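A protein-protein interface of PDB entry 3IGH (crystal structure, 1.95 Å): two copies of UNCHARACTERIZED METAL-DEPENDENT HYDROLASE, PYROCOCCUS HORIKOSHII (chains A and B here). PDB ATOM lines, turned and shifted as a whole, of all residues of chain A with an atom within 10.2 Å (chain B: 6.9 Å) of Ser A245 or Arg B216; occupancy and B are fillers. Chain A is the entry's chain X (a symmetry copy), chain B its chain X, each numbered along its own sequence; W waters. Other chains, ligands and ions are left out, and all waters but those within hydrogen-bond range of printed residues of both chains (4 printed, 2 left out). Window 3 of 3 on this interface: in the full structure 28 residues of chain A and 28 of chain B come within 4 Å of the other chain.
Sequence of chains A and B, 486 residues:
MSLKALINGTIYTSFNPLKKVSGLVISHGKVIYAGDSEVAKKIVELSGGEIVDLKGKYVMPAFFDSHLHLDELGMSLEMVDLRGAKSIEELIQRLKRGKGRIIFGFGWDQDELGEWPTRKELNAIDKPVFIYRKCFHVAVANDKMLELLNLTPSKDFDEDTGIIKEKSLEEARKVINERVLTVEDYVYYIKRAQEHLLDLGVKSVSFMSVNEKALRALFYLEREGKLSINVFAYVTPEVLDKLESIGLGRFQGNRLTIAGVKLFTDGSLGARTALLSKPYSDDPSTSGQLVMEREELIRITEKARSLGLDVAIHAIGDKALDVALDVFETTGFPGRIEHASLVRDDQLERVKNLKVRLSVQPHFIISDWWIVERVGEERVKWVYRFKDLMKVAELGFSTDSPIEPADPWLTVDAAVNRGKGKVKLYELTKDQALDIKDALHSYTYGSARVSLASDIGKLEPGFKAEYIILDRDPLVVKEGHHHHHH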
ATOM      1  N   LEU A 215      12.066 -10.202  32.587  1.00  0.00           N
ATOM      2  CA  LEU A 215      11.807  -9.300  31.467  1.00  0.00           C
ATOM      3  C   LEU A 215      12.523  -9.735  30.188  1.00  0.00           C
ATOM      4  O   LEU A 215      11.909  -9.739  29.126  1.00  0.00           O
ATOM      5  CB  LEU A 215      12.115  -7.836  31.813  1.00  0.00           C
ATOM      6  CG  LEU A 215      11.727  -6.815  30.718  1.00  0.00           C
ATOM      7  CD1 LEU A 215      10.240  -6.906  30.323  1.00  0.00           C
ATOM      8  CD2 LEU A 215      12.097  -5.391  31.107  1.00  0.00           C
ATOM      9  N   PRO A 237      11.095  -1.706  40.722  1.00  0.00           N
ATOM     10  CA  PRO A 237      11.776  -0.402  40.620  1.00  0.00           C
ATOM     11  C   PRO A 237      13.165  -0.441  39.974  1.00  0.00           C
ATOM     12  O   PRO A 237      13.538   0.504  39.280  1.00  0.00           O
ATOM     13  CB  PRO A 237      11.903   0.039  42.082  1.00  0.00           C
ATOM     14  CG  PRO A 237      10.716  -0.576  42.751  1.00  0.00           C
ATOM     15  CD  PRO A 237      10.586  -1.941  42.089  1.00  0.00           C
ATOM     16  N   GLU A 238      13.915  -1.517  40.203  1.00  0.00           N
ATOM     17  CA  GLU A 238      15.240  -1.670  39.628  1.00  0.00           C
ATOM     18  C   GLU A 238      15.147  -1.796  38.108  1.00  0.00           C
ATOM     19  O   GLU A 238      15.938  -1.188  37.379  1.00  0.00           O
ATOM     20  CB  GLU A 238      15.959  -2.883  40.239  1.00  0.00           C
ATOM     21  CG  GLU A 238      16.325  -2.736  41.732  1.00  0.00           C
ATOM     22  CD  GLU A 238      15.138  -2.855  42.721  1.00  0.00           C
ATOM     23  OE1 GLU A 238      15.300  -2.387  43.870  1.00  0.00           O
ATOM     24  OE2 GLU A 238      14.055  -3.397  42.372  1.00  0.00           O
ATOM     25  N   VAL A 239      14.171  -2.560  37.626  1.00  0.00           N
ATOM     26  CA  VAL A 239      13.939  -2.647  36.183  1.00  0.00           C
ATOM     27  C   VAL A 239      13.425  -1.332  35.600  1.00  0.00           C
ATOM     28  O   VAL A 239      13.827  -0.948  34.499  1.00  0.00           O
ATOM     29  CB  VAL A 239      13.015  -3.834  35.809  1.00  0.00           C
ATOM     30  CG1 VAL A 239      12.661  -3.811  34.324  1.00  0.00           C
ATOM     31  CG2 VAL A 239      13.720  -5.124  36.131  1.00  0.00           C
ATOM     32  N   LEU A 240      12.578  -0.630  36.349  1.00  0.00           N
ATOM     33  CA  LEU A 240      12.064   0.664  35.905  1.00  0.00           C
ATOM     34  C   LEU A 240      13.215   1.639  35.592  1.00  0.00           C
ATOM     35  O   LEU A 240      13.172   2.347  34.578  1.00  0.00           O
ATOM     36  CB  LEU A 240      11.100   1.262  36.942  1.00  0.00           C
ATOM     37  CG  LEU A 240      10.641   2.710  36.726  1.00  0.00           C
ATOM     38  CD1 LEU A 240       9.886   2.842  35.396  1.00  0.00           C
ATOM     39  CD2 LEU A 240       9.772   3.204  37.892  1.00  0.00           C
ATOM     40  N   ASP A 241      14.253   1.641  36.432  1.00  0.00           N
ATOM     41  CA  ASP A 241      15.458   2.462  36.162  1.00  0.00           C
ATOM     42  C   ASP A 241      16.069   2.164  34.798  1.00  0.00           C
ATOM     43  O   ASP A 241      16.518   3.067  34.094  1.00  0.00           O
ATOM     44  CB  ASP A 241      16.527   2.244  37.236  1.00  0.00           C
ATOM     45  CG  ASP A 241      16.166   2.882  38.563  1.00  0.00           C
ATOM     46  OD1 ASP A 241      15.235   3.717  38.596  1.00  0.00           O
ATOM     47  OD2 ASP A 241      16.817   2.544  39.576  1.00  0.00           O
ATOM     48  N   LYS A 242      16.090   0.887  34.436  1.00  0.00           N
ATOM     49  CA  LYS A 242      16.636   0.474  33.149  1.00  0.00           C
ATOM     50  C   LYS A 242      15.720   0.837  31.980  1.00  0.00           C
ATOM     51  O   LYS A 242      16.207   1.195  30.911  1.00  0.00           O
ATOM     52  CB  LYS A 242      16.957  -1.014  33.162  1.00  0.00           C
ATOM     53  CG  LYS A 242      18.060  -1.371  34.145  1.00  0.00           C
ATOM     54  CD  LYS A 242      18.581  -2.777  33.915  1.00  0.00           C
ATOM     55  CE  LYS A 242      19.802  -3.045  34.786  1.00  0.00           C
ATOM     56  NZ  LYS A 242      20.401  -4.382  34.525  1.00  0.00           N
ATOM     57  N   LEU A 243      14.403   0.766  32.185  1.00  0.00           N
ATOM     58  CA  LEU A 243      13.449   1.246  31.172  1.00  0.00           C
ATOM     59  C   LEU A 243      13.661   2.721  30.892  1.00  0.00           C
ATOM     60  O   LEU A 243      13.724   3.132  29.735  1.00  0.00           O
ATOM     61  CB  LEU A 243      12.005   1.028  31.626  1.00  0.00           C
ATOM     62  CG  LEU A 243      11.546  -0.417  31.843  1.00  0.00           C
ATOM     63  CD1 LEU A 243      10.059  -0.433  32.181  1.00  0.00           C
ATOM     64  CD2 LEU A 243      11.837  -1.282  30.623  1.00  0.00           C
ATOM     65  N   GLU A 244      13.766   3.502  31.969  1.00  0.00           N
ATOM     66  CA  GLU A 244      14.000   4.947  31.902  1.00  0.00           C
ATOM     67  C   GLU A 244      15.260   5.309  31.109  1.00  0.00           C
ATOM     68  O   GLU A 244      15.264   6.292  30.372  1.00  0.00           O
ATOM     69  CB  GLU A 244      14.031   5.528  33.325  1.00  0.00           C
ATOM     70  CG  GLU A 244      14.884   6.779  33.549  1.00  0.00           C
ATOM     71  CD  GLU A 244      14.127   8.070  33.344  1.00  0.00           C
ATOM     72  OE1 GLU A 244      13.674   8.330  32.209  1.00  0.00           O
ATOM     73  OE2 GLU A 244      14.000   8.837  34.325  1.00  0.00           O
ATOM     74  N   SER A 245      16.306   4.496  31.234  1.00  0.00           N
ATOM     75  CA  SER A 245      17.566   4.716  30.516  1.00  0.00           C
ATOM     76  C   SER A 245      17.450   4.706  28.981  1.00  0.00           C
ATOM     77  O   SER A 245      18.288   5.286  28.305  1.00  0.00           O
ATOM     78  CB  SER A 245      18.628   3.707  30.962  1.00  0.00           C
ATOM     79  OG  SER A 245      18.446   2.455  30.309  1.00  0.00           O
ATOM     80  N   ILE A 246      16.439   4.038  28.433  1.00  0.00           N
ATOM     81  CA  ILE A 246      16.175   4.128  26.994  1.00  0.00           C
ATOM     82  C   ILE A 246      14.882   4.869  26.664  1.00  0.00           C
ATOM     83  O   ILE A 246      14.560   5.076  25.494  1.00  0.00           O
ATOM     84  CB  ILE A 246      16.207   2.752  26.275  1.00  0.00           C
ATOM     85  CG1 ILE A 246      15.113   1.812  26.795  1.00  0.00           C
ATOM     86  CG2 ILE A 246      17.584   2.128  26.402  1.00  0.00           C
ATOM     87  CD1 ILE A 246      14.872   0.587  25.897  1.00  0.00           C
ATOM     88  N   GLY A 247      14.145   5.271  27.696  1.00  0.00           N
ATOM     89  CA  GLY A 247      12.894   5.999  27.498  1.00  0.00           C
ATOM     90  C   GLY A 247      11.728   5.077  27.179  1.00  0.00           C
ATOM     91  O   GLY A 247      10.703   5.524  26.675  1.00  0.00           O
ATOM     92  N   LEU A 248      11.871   3.790  27.494  1.00  0.00           N
ATOM     93  CA  LEU A 248      10.783   2.842  27.256  1.00  0.00           C
ATOM     94  C   LEU A 248       9.723   2.962  28.353  1.00  0.00           C
ATOM     95  O   LEU A 248       9.998   2.677  29.522  1.00  0.00           O
ATOM     96  CB  LEU A 248      11.317   1.405  27.161  1.00  0.00           C
ATOM     97  CG  LEU A 248      10.302   0.249  27.021  1.00  0.00           C
ATOM     98  CD1 LEU A 248       9.394   0.473  25.824  1.00  0.00           C
ATOM     99  CD2 LEU A 248      11.013  -1.101  26.884  1.00  0.00           C
ATOM    100  N   GLY A 249       8.520   3.387  27.968  1.00  0.00           N
ATOM    101  CA  GLY A 249       7.388   3.430  28.887  1.00  0.00           C
ATOM    102  C   GLY A 249       6.338   2.403  28.511  1.00  0.00           C
ATOM    103  O   GLY A 249       6.689   1.282  28.098  1.00  0.00           O
ATOM    104  N   ARG A 250       5.051   2.751  28.638  1.00  0.00           N
ATOM    105  CA  ARG A 250       4.009   1.812  28.213  1.00  0.00           C
ATOM    106  C   ARG A 250       4.211   1.466  26.744  1.00  0.00           C
ATOM    107  O   ARG A 250       4.441   2.347  25.904  1.00  0.00           O
ATOM    108  CB  ARG A 250       2.579   2.308  28.484  1.00  0.00           C
ATOM    109  CG  ARG A 250       1.546   1.174  28.338  1.00  0.00           C
ATOM    110  CD  ARG A 250       0.214   1.442  29.013  1.00  0.00           C
ATOM    111  NE  ARG A 250      -0.545   0.204  29.232  1.00  0.00           N
ATOM    112  CZ  ARG A 250      -0.818  -0.316  30.430  1.00  0.00           C
ATOM    113  NH1 ARG A 250      -0.410   0.295  31.538  1.00  0.00           N
ATOM    114  NH2 ARG A 250      -1.516  -1.447  30.525  1.00  0.00           N
ATOM    115  N   LYS A 303       8.510   8.787  38.475  1.00  0.00           N
ATOM    116  CA  LYS A 303       9.374   8.226  37.443  1.00  0.00           C
ATOM    117  C   LYS A 303       8.540   7.392  36.456  1.00  0.00           C
ATOM    118  O   LYS A 303       8.641   7.554  35.231  1.00  0.00           O
ATOM    119  CB  LYS A 303      10.458   7.369  38.096  1.00  0.00           C
ATOM    120  CG  LYS A 303      11.494   6.804  37.131  1.00  0.00           C
ATOM    121  CD  LYS A 303      12.471   5.859  37.840  1.00  0.00           C
ATOM    122  CE  LYS A 303      13.357   6.585  38.849  1.00  0.00           C
ATOM    123  NZ  LYS A 303      14.153   7.662  38.196  1.00  0.00           N
ATOM    124  N   SER A 306       6.144   9.599  34.343  1.00  0.00           N
ATOM    125  CA  SER A 306       6.891  10.294  33.294  1.00  0.00           C
ATOM    126  C   SER A 306       7.066   9.412  32.050  1.00  0.00           C
ATOM    127  O   SER A 306       7.386   9.914  30.977  1.00  0.00           O
ATOM    128  CB  SER A 306       8.254  10.789  33.810  1.00  0.00           C
ATOM    129  OG  SER A 306       9.237   9.758  33.833  1.00  0.00           O
ATOM    130  N   LEU A 307       6.826   8.109  32.206  1.00  0.00           N
ATOM    131  CA  LEU A 307       6.902   7.139  31.101  1.00  0.00           C
ATOM    132  C   LEU A 307       5.536   6.585  30.718  1.00  0.00           C
ATOM    133  O   LEU A 307       5.449   5.630  29.942  1.00  0.00           O
ATOM    134  CB  LEU A 307       7.871   5.999  31.463  1.00  0.00           C
ATOM    135  CG  LEU A 307       9.358   6.357  31.556  1.00  0.00           C
ATOM    136  CD1 LEU A 307      10.128   5.270  32.307  1.00  0.00           C
ATOM    137  CD2 LEU A 307       9.968   6.606  30.168  1.00  0.00           C
ATOM    138  N   GLY A 308       4.474   7.179  31.265  1.00  0.00           N
ATOM    139  CA  GLY A 308       3.098   6.739  31.006  1.00  0.00           C
ATOM    140  C   GLY A 308       2.793   5.345  31.538  1.00  0.00           C
ATOM    141  O   GLY A 308       1.864   4.686  31.070  1.00  0.00           O
ATOM    142  N   LEU A 309       3.590   4.894  32.503  1.00  0.00           N
ATOM    143  CA  LEU A 309       3.432   3.562  33.087  1.00  0.00           C
ATOM    144  C   LEU A 309       2.459   3.567  34.251  1.00  0.00           C
ATOM    145  O   LEU A 309       2.354   4.563  34.986  1.00  0.00           O
ATOM    146  CB  LEU A 309       4.791   3.013  33.541  1.00  0.00           C
ATOM    147  CG  LEU A 309       5.748   2.559  32.439  1.00  0.00           C
ATOM    148  CD1 LEU A 309       7.142   2.442  32.997  1.00  0.00           C
ATOM    149  CD2 LEU A 309       5.300   1.227  31.809  1.00  0.00           C
ATOM    150  N   VAL B 183      15.117  15.831  23.943  1.00  0.00           N
ATOM    151  CA  VAL B 183      14.068  14.910  23.496  1.00  0.00           C
ATOM    152  C   VAL B 183      12.864  15.665  22.919  1.00  0.00           C
ATOM    153  O   VAL B 183      12.324  15.269  21.875  1.00  0.00           O
ATOM    154  CB  VAL B 183      13.635  13.922  24.619  1.00  0.00           C
ATOM    155  CG1 VAL B 183      12.462  13.046  24.165  1.00  0.00           C
ATOM    156  CG2 VAL B 183      14.818  13.049  25.013  1.00  0.00           C
ATOM    157  N   TYR B 186      13.481  16.584  19.372  1.00  0.00           N
ATOM    158  CA  TYR B 186      13.297  15.396  18.533  1.00  0.00           C
ATOM    159  C   TYR B 186      11.825  15.067  18.321  1.00  0.00           C
ATOM    160  O   TYR B 186      11.437  14.714  17.207  1.00  0.00           O
ATOM    161  CB  TYR B 186      14.031  14.190  19.109  1.00  0.00           C
ATOM    162  CG  TYR B 186      15.509  14.121  18.788  1.00  0.00           C
ATOM    163  CD1 TYR B 186      16.455  14.703  19.636  1.00  0.00           C
ATOM    164  CD2 TYR B 186      15.964  13.458  17.648  1.00  0.00           C
ATOM    165  CE1 TYR B 186      17.820  14.626  19.354  1.00  0.00           C
ATOM    166  CE2 TYR B 186      17.322  13.383  17.349  1.00  0.00           C
ATOM    167  CZ  TYR B 186      18.237  13.970  18.208  1.00  0.00           C
ATOM    168  OH  TYR B 186      19.570  13.884  17.933  1.00  0.00           O
ATOM    169  N   VAL B 187      11.007  15.199  19.368  1.00  0.00           N
ATOM    170  CA  VAL B 187       9.554  14.992  19.237  1.00  0.00           C
ATOM    171  C   VAL B 187       8.992  15.971  18.190  1.00  0.00           C
ATOM    172  O   VAL B 187       8.259  15.571  17.292  1.00  0.00           O
ATOM    173  CB  VAL B 187       8.795  15.108  20.609  1.00  0.00           C
ATOM    174  CG1 VAL B 187       7.282  15.125  20.427  1.00  0.00           C
ATOM    175  CG2 VAL B 187       9.182  13.964  21.545  1.00  0.00           C
ATOM    176  N   VAL B 210      18.628   5.516  14.275  1.00  0.00           N
ATOM    177  CA  VAL B 210      17.891   6.104  15.384  1.00  0.00           C
ATOM    178  C   VAL B 210      18.852   6.161  16.573  1.00  0.00           C
ATOM    179  O   VAL B 210      19.330   5.117  17.037  1.00  0.00           O
ATOM    180  CB  VAL B 210      16.632   5.238  15.728  1.00  0.00           C
ATOM    181  CG1 VAL B 210      15.897   5.779  16.946  1.00  0.00           C
ATOM    182  CG2 VAL B 210      15.695   5.176  14.543  1.00  0.00           C
ATOM    183  N   ASN B 211      19.153   7.370  17.051  1.00  0.00           N
ATOM    184  CA  ASN B 211      20.020   7.529  18.220  1.00  0.00           C
ATOM    185  C   ASN B 211      19.213   7.510  19.528  1.00  0.00           C
ATOM    186  O   ASN B 211      18.015   7.229  19.515  1.00  0.00           O
ATOM    187  CB  ASN B 211      20.920   8.788  18.103  1.00  0.00           C
ATOM    188  CG  ASN B 211      20.132  10.104  18.054  1.00  0.00           C
ATOM    189  OD1 ASN B 211      19.045  10.228  18.622  1.00  0.00           O
ATOM    190  ND2 ASN B 211      20.701  11.105  17.373  1.00  0.00           N
ATOM    191  N   GLU B 212      19.868   7.826  20.643  1.00  0.00           N
ATOM    192  CA  GLU B 212      19.265   7.674  21.977  1.00  0.00           C
ATOM    193  C   GLU B 212      18.051   8.570  22.170  1.00  0.00           C
ATOM    194  O   GLU B 212      16.985   8.107  22.583  1.00  0.00           O
ATOM    195  CB  GLU B 212      20.305   7.955  23.079  1.00  0.00           C
ATOM    196  CG  GLU B 212      21.382   6.869  23.260  1.00  0.00           C
ATOM    197  CD  GLU B 212      22.592   6.978  22.305  1.00  0.00           C
ATOM    198  OE1 GLU B 212      22.565   7.743  21.299  1.00  0.00           O
ATOM    199  OE2 GLU B 212      23.589   6.268  22.578  1.00  0.00           O
ATOM    200  N   LYS B 213      18.203   9.849  21.841  1.00  0.00           N
ATOM    201  CA  LYS B 213      17.095  10.795  21.992  1.00  0.00           C
ATOM    202  C   LYS B 213      15.974  10.642  20.973  1.00  0.00           C
ATOM    203  O   LYS B 213      14.806  10.889  21.297  1.00  0.00           O
ATOM    204  CB  LYS B 213      17.610  12.228  22.016  1.00  0.00           C
ATOM    205  CG  LYS B 213      18.401  12.535  23.256  1.00  0.00           C
ATOM    206  CD  LYS B 213      18.759  13.996  23.356  1.00  0.00           C
ATOM    207  CE  LYS B 213      19.486  14.250  24.667  1.00  0.00           C
ATOM    208  NZ  LYS B 213      20.033  15.626  24.740  1.00  0.00           N
ATOM    209  N   ALA B 214      16.320  10.265  19.742  1.00  0.00           N
ATOM    210  CA  ALA B 214      15.303   9.959  18.731  1.00  0.00           C
ATOM    211  C   ALA B 214      14.473   8.758  19.192  1.00  0.00           C
ATOM    212  O   ALA B 214      13.259   8.762  19.045  1.00  0.00           O
ATOM    213  CB  ALA B 214      15.930   9.675  17.372  1.00  0.00           C
ATOM    214  N   LEU B 215      15.134   7.749  19.763  1.00  0.00           N
ATOM    215  CA  LEU B 215      14.410   6.599  20.301  1.00  0.00           C
ATOM    216  C   LEU B 215      13.480   6.980  21.453  1.00  0.00           C
ATOM    217  O   LEU B 215      12.335   6.540  21.474  1.00  0.00           O
ATOM    218  CB  LEU B 215      15.350   5.450  20.694  1.00  0.00           C
ATOM    219  CG  LEU B 215      14.637   4.151  21.136  1.00  0.00           C
ATOM    220  CD1 LEU B 215      13.658   3.620  20.071  1.00  0.00           C
ATOM    221  CD2 LEU B 215      15.623   3.069  21.551  1.00  0.00           C
ATOM    222  N   ARG B 216      13.953   7.812  22.385  1.00  0.00           N
ATOM    223  CA  ARG B 216      13.086   8.317  23.468  1.00  0.00           C
ATOM    224  C   ARG B 216      11.857   9.049  22.926  1.00  0.00           C
ATOM    225  O   ARG B 216      10.749   8.881  23.437  1.00  0.00           O
ATOM    226  CB  ARG B 216      13.850   9.260  24.399  1.00  0.00           C
ATOM    227  CG  ARG B 216      14.887   8.597  25.271  1.00  0.00           C
ATOM    228  CD  ARG B 216      15.456   9.647  26.222  1.00  0.00           C
ATOM    229  NE  ARG B 216      16.455   9.084  27.111  1.00  0.00           N
ATOM    230  CZ  ARG B 216      16.182   8.572  28.306  1.00  0.00           C
ATOM    231  NH1 ARG B 216      17.161   8.078  29.047  1.00  0.00           N
ATOM    232  NH2 ARG B 216      14.932   8.557  28.760  1.00  0.00           N
ATOM    233  N   ALA B 217      12.072   9.867  21.897  1.00  0.00           N
ATOM    234  CA  ALA B 217      11.000  10.604  21.235  1.00  0.00           C
ATOM    235  C   ALA B 217       9.992   9.654  20.582  1.00  0.00           C
ATOM    236  O   ALA B 217       8.778   9.840  20.699  1.00  0.00           O
ATOM    237  CB  ALA B 217      11.590  11.550  20.190  1.00  0.00           C
ATOM    238  N   LEU B 218      10.503   8.641  19.888  1.00  0.00           N
ATOM    239  CA  LEU B 218       9.642   7.645  19.243  1.00  0.00           C
ATOM    240  C   LEU B 218       8.772   6.885  20.242  1.00  0.00           C
ATOM    241  O   LEU B 218       7.571   6.712  20.005  1.00  0.00           O
ATOM    242  CB  LEU B 218      10.467   6.668  18.391  1.00  0.00           C
ATOM    243  CG  LEU B 218      11.079   7.191  17.082  1.00  0.00           C
ATOM    244  CD1 LEU B 218      12.055   6.164  16.518  1.00  0.00           C
ATOM    245  CD2 LEU B 218       9.994   7.561  16.048  1.00  0.00           C
ATOM    246  N   PHE B 219       9.381   6.446  21.350  1.00  0.00           N
ATOM    247  CA  PHE B 219       8.657   5.798  22.451  1.00  0.00           C
ATOM    248  C   PHE B 219       7.556   6.712  23.012  1.00  0.00           C
ATOM    249  O   PHE B 219       6.441   6.267  23.253  1.00  0.00           O
ATOM    250  CB  PHE B 219       9.614   5.390  23.588  1.00  0.00           C
ATOM    251  CG  PHE B 219      10.375   4.109  23.339  1.00  0.00           C
ATOM    252  CD1 PHE B 219       9.750   2.994  22.766  1.00  0.00           C
ATOM    253  CD2 PHE B 219      11.701   4.000  23.724  1.00  0.00           C
ATOM    254  CE1 PHE B 219      10.459   1.800  22.551  1.00  0.00           C
ATOM    255  CE2 PHE B 219      12.416   2.816  23.520  1.00  0.00           C
ATOM    256  CZ  PHE B 219      11.794   1.713  22.927  1.00  0.00           C
ATOM    257  N   TYR B 220       7.883   7.988  23.207  1.00  0.00           N
ATOM    258  CA  TYR B 220       6.907   8.982  23.664  1.00  0.00           C
ATOM    259  C   TYR B 220       5.713   9.085  22.705  1.00  0.00           C
ATOM    260  O   TYR B 220       4.561   8.963  23.119  1.00  0.00           O
ATOM    261  CB  TYR B 220       7.585  10.357  23.823  1.00  0.00           C
ATOM    262  CG  TYR B 220       6.605  11.474  24.105  1.00  0.00           C
ATOM    263  CD1 TYR B 220       6.095  11.675  25.391  1.00  0.00           C
ATOM    264  CD2 TYR B 220       6.170  12.325  23.079  1.00  0.00           C
ATOM    265  CE1 TYR B 220       5.184  12.700  25.650  1.00  0.00           C
ATOM    266  CE2 TYR B 220       5.259  13.340  23.325  1.00  0.00           C
ATOM    267  CZ  TYR B 220       4.778  13.528  24.616  1.00  0.00           C
ATOM    268  OH  TYR B 220       3.878  14.535  24.860  1.00  0.00           O
ATOM    269  N   LEU B 221       6.001   9.290  21.421  1.00  0.00           N
ATOM    270  CA  LEU B 221       4.952   9.439  20.410  1.00  0.00           C
ATOM    271  C   LEU B 221       4.067   8.208  20.281  1.00  0.00           C
ATOM    272  O   LEU B 221       2.856   8.335  20.152  1.00  0.00           O
ATOM    273  CB  LEU B 221       5.562   9.793  19.052  1.00  0.00           C
ATOM    274  CG  LEU B 221       6.118  11.217  18.921  1.00  0.00           C
ATOM    275  CD1 LEU B 221       6.899  11.332  17.646  1.00  0.00           C
ATOM    276  CD2 LEU B 221       5.001  12.271  18.960  1.00  0.00           C
ATOM    277  N   LYS B 242      22.304  -0.517  24.545  1.00  0.00           N
ATOM    278  CA  LYS B 242      21.304  -0.218  25.563  1.00  0.00           C
ATOM    279  C   LYS B 242      20.075  -1.122  25.462  1.00  0.00           C
ATOM    280  O   LYS B 242      19.510  -1.500  26.483  1.00  0.00           O
ATOM    281  CB  LYS B 242      20.918   1.253  25.511  1.00  0.00           C
ATOM    282  CG  LYS B 242      22.070   2.179  25.864  1.00  0.00           C
ATOM    283  CD  LYS B 242      21.591   3.596  26.119  1.00  0.00           C
ATOM    284  CE  LYS B 242      22.730   4.459  26.647  1.00  0.00           C
ATOM    285  NZ  LYS B 242      22.283   5.835  26.998  1.00  0.00           N
ATOM    286  N   SER B 245      20.998  -4.400  27.102  1.00  0.00           N
ATOM    287  CA  SER B 245      20.996  -4.303  28.565  1.00  0.00           C
ATOM    288  C   SER B 245      19.659  -4.660  29.239  1.00  0.00           C
ATOM    289  O   SER B 245      19.647  -5.031  30.404  1.00  0.00           O
ATOM    290  CB  SER B 245      21.449  -2.912  29.016  1.00  0.00           C
ATOM    291  OG  SER B 245      20.381  -1.975  28.928  1.00  0.00           O
ATOM    292  N   ILE B 246      18.543  -4.528  28.527  1.00  0.00           N
ATOM    293  CA  ILE B 246      17.261  -5.008  29.050  1.00  0.00           C
ATOM    294  C   ILE B 246      16.715  -6.214  28.290  1.00  0.00           C
ATOM    295  O   ILE B 246      15.675  -6.764  28.654  1.00  0.00           O
ATOM    296  CB  ILE B 246      16.181  -3.896  29.149  1.00  0.00           C
ATOM    297  CG1 ILE B 246      15.829  -3.321  27.772  1.00  0.00           C
ATOM    298  CG2 ILE B 246      16.636  -2.811  30.106  1.00  0.00           C
ATOM    299  CD1 ILE B 246      14.540  -2.483  27.764  1.00  0.00           C
HETATM  300  O   HOH W   1      17.084   5.747  24.122  1.00  0.00           O
HETATM  301  O   HOH W   2      19.114   6.204  25.775  1.00  0.00           O
HETATM  302  O   HOH W   3      10.421   8.255  26.107  1.00  0.00           O
HETATM  303  O   HOH W   4      18.198  -6.107  32.565  1.00  0.00           O
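OE1 of Glu A244 lies within salt-bridge range of NH2 of Arg B216 (3.7 Å). O of Ser A245 lies within hydrogen-bond range of NH1 of Arg B216, at 3.1 Å.
The backbone carbonyl oxygen of Lys B242 sits at hydrogen-bond distance from the side-chain hydroxyl of Ser B245. O of Lys A242 sits at hydrogen-bond distance from OG of Ser A245 (2.6 Å). O of Leu A243 lies within hydrogen-bond range of N of Leu A248 (3.0 Å).
Among the printed residues, pairs that only touch across the chains: Lys A242 with Ile B246 (3.6 Å), Ile A246 with Arg B216 (3.5 Å), Ile A246 with Phe B219 (3.5 Å), Ile A246 with Lys B242 (3.6 Å), Ile A246 with Ile B246 (3.6 Å), Gly A247 with Arg B216 (3.5 Å), Gly A247 with Phe B219 (3.3 Å), Leu A248 with Phe B219 (3.7 Å) and Leu A248 with Ile B246 (3.9 Å).
Printed residues of chain B within 4 Å of Glu A244: Arg B216 (2.8 Å). Of chain B, only Arg B216 (3.1 Å) comes within 4 Å of Ser A245. No residue of chain A comes within 4 Å of Ala B214. No residue of chain A comes within 4 Å of Leu B215. Arg B216 touches four residues of chain A. No residue of chain A comes within 4 Å of Ala B217. Leu B221 touches none of the printed residues of chain A. Of the printed residues of chain A, Lys B242 touches Ile A246 (3.6 Å). Printed residues of chain A within 4 Å of Ile B246: Lys A242, Ile A246 and Leu A248.
Of the 18 printed residues of chain B, 4 touch a printed residue of chain A. Hydrophobic or aromatic side chains of chain B within 4 Å of the printed part of chain A: Phe B219 and Ile B246. Of the 20 printed residues of chain A, 6 touch a printed residue of chain B. Among the printed residues, 11 pairs touch across the chains.
Lys A242 touches Ile B246, and with the chains exchanged Ile A246 touches Lys B242. Ile A246 touches its own counterpart, Ile B246. Of the 11 pairs that touch across the chains among the printed residues, 3 have their exchanged pair printed and touching as well.
Water W3 bridges O of Arg B216 and O of Gly A247. Water W2 bridges the backbone carbonyl oxygen of Ser A245 (2.8 Å) and the side-chain amino group of Lys B242 (3.4 Å). Water W4 lies within hydrogen-bond range of the backbone carbonyl oxygen of Ser B245 (2.8 Å) and the side-chain amino group of Lys A242 (3.4 Å). Water W1 lies within hydrogen-bond range of O of Glu B212 (2.8 Å) and O of Ile A246 (3.0 Å).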
